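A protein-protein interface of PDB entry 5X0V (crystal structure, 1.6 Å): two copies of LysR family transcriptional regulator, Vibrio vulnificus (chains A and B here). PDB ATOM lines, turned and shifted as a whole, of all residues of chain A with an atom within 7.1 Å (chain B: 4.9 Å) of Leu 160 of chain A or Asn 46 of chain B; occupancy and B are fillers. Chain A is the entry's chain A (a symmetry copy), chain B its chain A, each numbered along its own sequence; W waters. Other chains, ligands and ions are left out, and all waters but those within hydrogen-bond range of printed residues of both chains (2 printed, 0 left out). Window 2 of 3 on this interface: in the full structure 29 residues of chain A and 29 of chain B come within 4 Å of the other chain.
The side-chain amide nitrogen (ND2) of Asn 158 of chain A sits close to the backbone NH (N) of Leu 47 of chain B, at 2.9 Å.
The backbone carbonyl oxygen (O) of Leu 18 of chain B sits at hydrogen-bond distance from the backbone NH (N) of Leu 48 of chain B (2.9 Å). The backbone NH (N) of Leu 160 of chain A lies within hydrogen-bond range of the backbone carbonyl oxygen (O) of Met 155 of chain A (3.3 Å). The backbone carbonyl oxygen (O) of Gly 16 of chain B sits at hydrogen-bond distance from the backbone NH (N) of Asn 46 of chain B, at 2.8 Å. The backbone NH (N) of Phe 117 of chain A is in hydrogen-bond range of the backbone carbonyl oxygen (O) of Thr 162 of chain A (3.0 Å). O of Asn 46 of chain B is in hydrogen-bond range of N of Leu 18 of chain B.
Leu 48 of chain B touches Phe 117 of chain A. Leu 47 of chain B touches Met 155 of chain A. Met 155 of chain A touches Leu 48 of chain B (SD to CA, 3.9 Å). OD1 of Asn 158 of chain A touches O of Leu 45 of chain B, at 3.7 Å. Asn 46 of chain B touches Asn 158 of chain A. CD2 of Leu 160 of chain A touches CG of Asn 46 of chain B (3.4 Å). CD1 of Leu 160 of chain A touches O of Leu 47 of chain B, at 3.5 Å. CD2 of Leu 48 of chain B touches CD1 of Leu 160 of chain A, at 3.96 Å.
Val 156 of chain A touches none of the printed residues of chain B. Asn 46 of chain B touches two residues of chain A. Printed residues of chain A within 4 Å of Leu 47 of chain B: Met 155 (3.5 Å), Asn 158 (2.9 Å) and Leu 160 (3.5 Å). Printed residues of chain A within 4 Å of Leu 48 of chain B: Phe 117 (3.9 Å), Met 155 (3.9 Å) and Leu 160 (3.96 Å). The nearest printed residue of chain B that does not touch Leu 160 of chain A is Leu 45 of chain B (5.5 Å).
Hydrophobic or aromatic side chains of chain A within 4 Å of the printed part of chain B: Phe 117, Met 155 and Leu 160. Hydrophobic or aromatic side chains of chain B within 4 Å of the printed part of chain A: Leu 47 and Leu 48. Among the printed residues, 9 pairs touch across the chains. Among the printed residues, no Asp or Glu carboxylate lies within 4 Å of a Lys or Arg side-chain nitrogen of the other chain.
No position is printed for both chains. Of the 9 pairs that touch across the chains among the printed residues, none has its exchanged pair printed and touching as well.
Water W1 lies within hydrogen-bond range of O of Leu 45 of chain B (2.7 Å) and OD1 of Asn 158 of chain A (3.3 Å). Water W2 bridges the side-chain amide nitrogen (NE2) of Gln 17 of chain B (3.3 Å) and the side-chain amide nitrogen (ND2) of Asn 142 of chain A (3.4 Å).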
ATOM      1  N   SER A  95      11.933 -21.278  -1.677  1.00  0.00           N
ATOM      2  CA  SER A  95      12.797 -22.456  -1.671  1.00  0.00           C
ATOM      3  C   SER A  95      12.363 -23.441  -0.593  1.00  0.00           C
ATOM      4  O   SER A  95      11.960 -23.050   0.505  1.00  0.00           O
ATOM      5  CB  SER A  95      14.248 -22.060  -1.461  1.00  0.00           C
ATOM      6  OG  SER A  95      15.032 -23.199  -1.144  1.00  0.00           O
ATOM      7  N   GLN A  98      13.807 -22.739   2.728  1.00  0.00           N
ATOM      8  CA  GLN A  98      13.282 -21.591   3.453  1.00  0.00           C
ATOM      9  C   GLN A  98      11.816 -21.778   3.802  1.00  0.00           C
ATOM     10  O   GLN A  98      11.230 -20.900   4.437  1.00  0.00           O
ATOM     11  CB  GLN A  98      13.430 -20.295   2.626  1.00  0.00           C
ATOM     12  CG  GLN A  98      14.846 -19.699   2.509  1.00  0.00           C
ATOM     13  CD  GLN A  98      15.282 -19.016   3.802  1.00  0.00           C
ATOM     14  OE1 GLN A  98      14.636 -19.165   4.836  1.00  0.00           O
ATOM     15  NE2 GLN A  98      16.370 -18.264   3.748  1.00  0.00           N
ATOM     16  N   GLU A 114      12.100  -6.546   2.317  1.00  0.00           N
ATOM     17  CA  GLU A 114      12.932  -6.784   1.136  1.00  0.00           C
ATOM     18  C   GLU A 114      12.982  -8.259   0.744  1.00  0.00           C
ATOM     19  O   GLU A 114      13.917  -8.701   0.072  1.00  0.00           O
ATOM     20  CB  GLU A 114      14.356  -6.233   1.308  1.00  0.00           C
ATOM     21  CG  GLU A 114      14.340  -4.725   1.442  1.00  0.00           C
ATOM     22  CD  GLU A 114      15.715  -4.114   1.523  1.00  0.00           C
ATOM     23  OE1 GLU A 114      15.778  -2.910   1.783  1.00  0.00           O
ATOM     24  OE2 GLU A 114      16.722  -4.809   1.327  1.00  0.00           O
ATOM     25  N   SER A 115      11.963  -9.034   1.119  1.00  0.00           N
ATOM     26  CA  SER A 115      11.989 -10.448   0.793  1.00  0.00           C
ATOM     27  C   SER A 115      11.254 -10.782  -0.506  1.00  0.00           C
ATOM     28  O   SER A 115      11.395 -11.900  -1.009  1.00  0.00           O
ATOM     29  CB  SER A 115      11.422 -11.265   1.971  1.00  0.00           C
ATOM     30  OG  SER A 115      10.067 -10.939   2.170  1.00  0.00           O
ATOM     31  N   VAL A 116      10.539  -9.841  -1.114  1.00  0.00           N
ATOM     32  CA  VAL A 116       9.798 -10.109  -2.356  1.00  0.00           C
ATOM     33  C   VAL A 116      10.572  -9.549  -3.539  1.00  0.00           C
ATOM     34  O   VAL A 116      10.777  -8.334  -3.636  1.00  0.00           O
ATOM     35  CB  VAL A 116       8.372  -9.537  -2.298  1.00  0.00           C
ATOM     36  CG1 VAL A 116       7.643  -9.909  -3.579  1.00  0.00           C
ATOM     37  CG2 VAL A 116       7.651 -10.153  -1.079  1.00  0.00           C
ATOM     38  N   PHE A 117      10.997 -10.435  -4.444  1.00  0.00           N
ATOM     39  CA  PHE A 117      11.692 -10.026  -5.662  1.00  0.00           C
ATOM     40  C   PHE A 117      10.680  -9.859  -6.778  1.00  0.00           C
ATOM     41  O   PHE A 117       9.747 -10.673  -6.901  1.00  0.00           O
ATOM     42  CB  PHE A 117      12.760 -11.092  -6.019  1.00  0.00           C
ATOM     43  CG  PHE A 117      13.974 -11.019  -5.134  1.00  0.00           C
ATOM     44  CD1 PHE A 117      13.953 -11.588  -3.857  1.00  0.00           C
ATOM     45  CD2 PHE A 117      15.133 -10.322  -5.557  1.00  0.00           C
ATOM     46  CE1 PHE A 117      15.062 -11.498  -2.995  1.00  0.00           C
ATOM     47  CE2 PHE A 117      16.252 -10.217  -4.694  1.00  0.00           C
ATOM     48  CZ  PHE A 117      16.206 -10.790  -3.417  1.00  0.00           C
ATOM     49  N   ASN A 142      12.164  -6.317  -2.528  1.00  0.00           N
ATOM     50  CA  ASN A 142      13.613  -6.176  -2.581  1.00  0.00           C
ATOM     51  C   ASN A 142      13.974  -5.082  -3.596  1.00  0.00           C
ATOM     52  O   ASN A 142      13.366  -5.026  -4.668  1.00  0.00           O
ATOM     53  CB  ASN A 142      14.282  -7.519  -2.976  1.00  0.00           C
ATOM     54  CG  ASN A 142      15.769  -7.485  -2.722  1.00  0.00           C
ATOM     55  OD1 ASN A 142      16.520  -6.900  -3.490  1.00  0.00           O
ATOM     56  ND2 ASN A 142      16.192  -7.996  -1.559  1.00  0.00           N
ATOM     57  N   GLN A 154      15.499 -18.363 -10.170  1.00  0.00           N
ATOM     58  CA  GLN A 154      16.790 -18.850  -9.668  1.00  0.00           C
ATOM     59  C   GLN A 154      17.182 -18.126  -8.395  1.00  0.00           C
ATOM     60  O   GLN A 154      17.696 -18.751  -7.458  1.00  0.00           O
ATOM     61  CB  GLN A 154      17.874 -18.665 -10.732  1.00  0.00           C
ATOM     62  CG  GLN A 154      17.714 -19.668 -11.899  1.00  0.00           C
ATOM     63  CD  GLN A 154      18.248 -19.172 -13.204  1.00  0.00           C
ATOM     64  OE1 GLN A 154      18.785 -18.080 -13.277  1.00  0.00           O
ATOM     65  NE2 GLN A 154      18.102 -19.999 -14.292  1.00  0.00           N
ATOM     66  N   MET A 155      16.947 -16.810  -8.320  1.00  0.00           N
ATOM     67  CA  MET A 155      17.241 -16.147  -7.044  1.00  0.00           C
ATOM     68  C   MET A 155      16.386 -16.711  -5.907  1.00  0.00           C
ATOM     69  O   MET A 155      16.855 -16.809  -4.772  1.00  0.00           O
ATOM     70  CB  MET A 155      17.021 -14.625  -7.127  1.00  0.00           C
ATOM     71  CG  MET A 155      18.122 -13.957  -7.993  1.00  0.00           C
ATOM     72  SD  MET A 155      18.036 -12.161  -7.937  1.00  0.00           S
ATOM     73  CE  MET A 155      16.607 -11.849  -9.016  1.00  0.00           C
ATOM     74  N   VAL A 156      15.111 -17.003  -6.161  1.00  0.00           N
ATOM     75  CA  VAL A 156      14.280 -17.556  -5.099  1.00  0.00           C
ATOM     76  C   VAL A 156      14.799 -18.939  -4.738  1.00  0.00           C
ATOM     77  O   VAL A 156      14.843 -19.325  -3.556  1.00  0.00           O
ATOM     78  CB  VAL A 156      12.799 -17.593  -5.560  1.00  0.00           C
ATOM     79  CG1 VAL A 156      11.935 -18.473  -4.598  1.00  0.00           C
ATOM     80  CG2 VAL A 156      12.188 -16.151  -5.602  1.00  0.00           C
ATOM     81  N   ALA A 157      15.216 -19.705  -5.754  1.00  0.00           N
ATOM     82  CA  ALA A 157      15.762 -21.040  -5.498  1.00  0.00           C
ATOM     83  C   ALA A 157      17.052 -20.965  -4.685  1.00  0.00           C
ATOM     84  O   ALA A 157      17.395 -21.921  -3.967  1.00  0.00           O
ATOM     85  CB  ALA A 157      16.030 -21.785  -6.828  1.00  0.00           C
ATOM     86  N   ASN A 158      17.792 -19.851  -4.788  1.00  0.00           N
ATOM     87  CA  ASN A 158      19.004 -19.650  -3.988  1.00  0.00           C
ATOM     88  C   ASN A 158      18.657 -19.264  -2.551  1.00  0.00           C
ATOM     89  O   ASN A 158      19.572 -19.108  -1.705  1.00  0.00           O
ATOM     90  CB  ASN A 158      19.848 -18.569  -4.730  1.00  0.00           C
ATOM     91  CG  ASN A 158      21.217 -18.332  -4.117  1.00  0.00           C
ATOM     92  OD1 ASN A 158      21.967 -19.270  -3.774  1.00  0.00           O
ATOM     93  ND2 ASN A 158      21.549 -17.086  -3.970  1.00  0.00           N
ATOM     94  N   GLY A 159      17.353 -19.162  -2.230  1.00  0.00           N
ATOM     95  CA  GLY A 159      16.911 -18.877  -0.871  1.00  0.00           C
ATOM     96  C   GLY A 159      16.750 -17.414  -0.524  1.00  0.00           C
ATOM     97  O   GLY A 159      16.587 -17.087   0.668  1.00  0.00           O
ATOM     98  N   LEU A 160      16.773 -16.521  -1.504  1.00  0.00           N
ATOM     99  CA  LEU A 160      16.855 -15.093  -1.196  1.00  0.00           C
ATOM    100  C   LEU A 160      15.518 -14.483  -0.801  1.00  0.00           C
ATOM    101  O   LEU A 160      15.506 -13.400  -0.197  1.00  0.00           O
ATOM    102  CB  LEU A 160      17.428 -14.353  -2.397  1.00  0.00           C
ATOM    103  CG  LEU A 160      18.820 -14.835  -2.899  1.00  0.00           C
ATOM    104  CD1 LEU A 160      19.388 -13.783  -3.852  1.00  0.00           C
ATOM    105  CD2 LEU A 160      19.814 -15.114  -1.722  1.00  0.00           C
ATOM    106  N   GLY A 161      14.399 -15.127  -1.123  1.00  0.00           N
ATOM    107  CA  GLY A 161      13.092 -14.596  -0.762  1.00  0.00           C
ATOM    108  C   GLY A 161      12.018 -15.327  -1.542  1.00  0.00           C
ATOM    109  O   GLY A 161      12.125 -16.537  -1.753  1.00  0.00           O
ATOM    110  N   THR A 162      10.991 -14.601  -1.970  1.00  0.00           N
ATOM    111  CA  THR A 162       9.821 -15.197  -2.603  1.00  0.00           C
ATOM    112  C   THR A 162       9.418 -14.331  -3.779  1.00  0.00           C
ATOM    113  O   THR A 162       9.921 -13.219  -3.954  1.00  0.00           O
ATOM    114  CB  THR A 162       8.661 -15.334  -1.585  1.00  0.00           C
ATOM    115  OG1 THR A 162       7.572 -16.044  -2.180  1.00  0.00           O
ATOM    116  CG2 THR A 162       8.165 -13.977  -1.033  1.00  0.00           C
ATOM    117  N   GLY B  16      28.583 -13.863   1.410  1.00  0.00           N
ATOM    118  CA  GLY B  16      28.062 -12.563   1.119  1.00  0.00           C
ATOM    119  C   GLY B  16      27.345 -12.541  -0.207  1.00  0.00           C
ATOM    120  O   GLY B  16      26.909 -13.556  -0.733  1.00  0.00           O
ATOM    121  N   GLN B  17      27.250 -11.350  -0.758  1.00  0.00           N
ATOM    122  CA  GLN B  17      26.435 -11.090  -1.925  1.00  0.00           C
ATOM    123  C   GLN B  17      27.326 -10.934  -3.155  1.00  0.00           C
ATOM    124  O   GLN B  17      28.406 -10.340  -3.082  1.00  0.00           O
ATOM    125  CB  GLN B  17      25.633  -9.842  -1.677  1.00  0.00           C
ATOM    126  CG  GLN B  17      24.605  -9.526  -2.678  1.00  0.00           C
ATOM    127  CD  GLN B  17      23.837  -8.322  -2.242  1.00  0.00           C
ATOM    128  OE1 GLN B  17      24.269  -7.186  -2.458  1.00  0.00           O
ATOM    129  NE2 GLN B  17      22.693  -8.551  -1.620  1.00  0.00           N
ATOM    130  N   LEU B  18      26.873 -11.451  -4.289  1.00  0.00           N
ATOM    131  CA  LEU B  18      27.555 -11.303  -5.562  1.00  0.00           C
ATOM    132  C   LEU B  18      26.510 -10.937  -6.613  1.00  0.00           C
ATOM    133  O   LEU B  18      25.503 -11.635  -6.738  1.00  0.00           O
ATOM    134  CB  LEU B  18      28.205 -12.620  -5.938  1.00  0.00           C
ATOM    135  CG  LEU B  18      29.377 -12.778  -6.865  1.00  0.00           C
ATOM    136  CD1 LEU B  18      30.572 -12.089  -6.244  1.00  0.00           C
ATOM    137  CD2 LEU B  18      29.613 -14.303  -7.062  1.00  0.00           C
ATOM    138  N   GLN B  44      26.435 -19.591   2.288  1.00  0.00           N
ATOM    139  CA  GLN B  44      26.346 -18.171   2.630  1.00  0.00           C
ATOM    140  C   GLN B  44      26.559 -17.236   1.448  1.00  0.00           C
ATOM    141  O   GLN B  44      26.679 -16.017   1.644  1.00  0.00           O
ATOM    142  CB  GLN B  44      27.338 -17.812   3.731  1.00  0.00           C
ATOM    143  CG  GLN B  44      26.775 -18.077   5.125  1.00  0.00           C
ATOM    144  CD  GLN B  44      27.004 -19.489   5.544  1.00  0.00           C
ATOM    145  OE1 GLN B  44      28.155 -19.917   5.708  1.00  0.00           O
ATOM    146  NE2 GLN B  44      25.917 -20.246   5.709  1.00  0.00           N
ATOM    147  N   LEU B  45      26.581 -17.751   0.236  1.00  0.00           N
ATOM    148  CA  LEU B  45      26.771 -16.943  -0.964  1.00  0.00           C
ATOM    149  C   LEU B  45      25.406 -16.644  -1.607  1.00  0.00           C
ATOM    150  O   LEU B  45      24.674 -17.573  -1.974  1.00  0.00           O
ATOM    151  CB  LEU B  45      27.645 -17.699  -1.965  1.00  0.00           C
ATOM    152  CG  LEU B  45      28.123 -16.827  -3.118  1.00  0.00           C
ATOM    153  CD1 LEU B  45      28.955 -15.702  -2.535  1.00  0.00           C
ATOM    154  CD2 LEU B  45      28.889 -17.649  -4.141  1.00  0.00           C
ATOM    155  N   ASN B  46      25.045 -15.368  -1.693  1.00  0.00           N
ATOM    156  CA  ASN B  46      23.755 -14.945  -2.215  1.00  0.00           C
ATOM    157  C   ASN B  46      24.020 -14.384  -3.593  1.00  0.00           C
ATOM    158  O   ASN B  46      24.878 -13.506  -3.730  1.00  0.00           O
ATOM    159  CB  ASN B  46      23.156 -13.872  -1.309  1.00  0.00           C
ATOM    160  CG  ASN B  46      22.666 -14.407   0.000  1.00  0.00           C
ATOM    161  OD1 ASN B  46      22.563 -15.624   0.224  1.00  0.00           O
ATOM    162  ND2 ASN B  46      22.363 -13.483   0.905  1.00  0.00           N
ATOM    163  N   LEU B  47      23.342 -14.926  -4.631  1.00  0.00           N
ATOM    164  CA  LEU B  47      23.603 -14.544  -6.008  1.00  0.00           C
ATOM    165  C   LEU B  47      22.473 -13.650  -6.497  1.00  0.00           C
ATOM    166  O   LEU B  47      21.370 -14.151  -6.736  1.00  0.00           O
ATOM    167  CB  LEU B  47      23.703 -15.790  -6.897  1.00  0.00           C
ATOM    168  CG  LEU B  47      24.906 -16.672  -6.882  1.00  0.00           C
ATOM    169  CD1 LEU B  47      24.810 -17.415  -8.216  1.00  0.00           C
ATOM    170  CD2 LEU B  47      26.210 -15.896  -6.777  1.00  0.00           C
ATOM    171  N   LEU B  48      22.731 -12.330  -6.663  1.00  0.00           N
ATOM    172  CA  LEU B  48      21.781 -11.445  -7.336  1.00  0.00           C
ATOM    173  C   LEU B  48      22.078 -11.571  -8.819  1.00  0.00           C
ATOM    174  O   LEU B  48      23.233 -11.482  -9.225  1.00  0.00           O
ATOM    175  CB  LEU B  48      21.922  -9.994  -6.868  1.00  0.00           C
ATOM    176  CG  LEU B  48      21.587  -9.793  -5.403  1.00  0.00           C
ATOM    177  CD1 LEU B  48      22.020  -8.400  -4.885  1.00  0.00           C
ATOM    178  CD2 LEU B  48      20.113 -10.085  -5.078  1.00  0.00           C
HETATM  179  O   HOH W   1      24.450 -20.306  -1.849  1.00  0.00           O
HETATM  180  O   HOH W   2      19.496  -8.344  -1.016  1.00  0.00           O
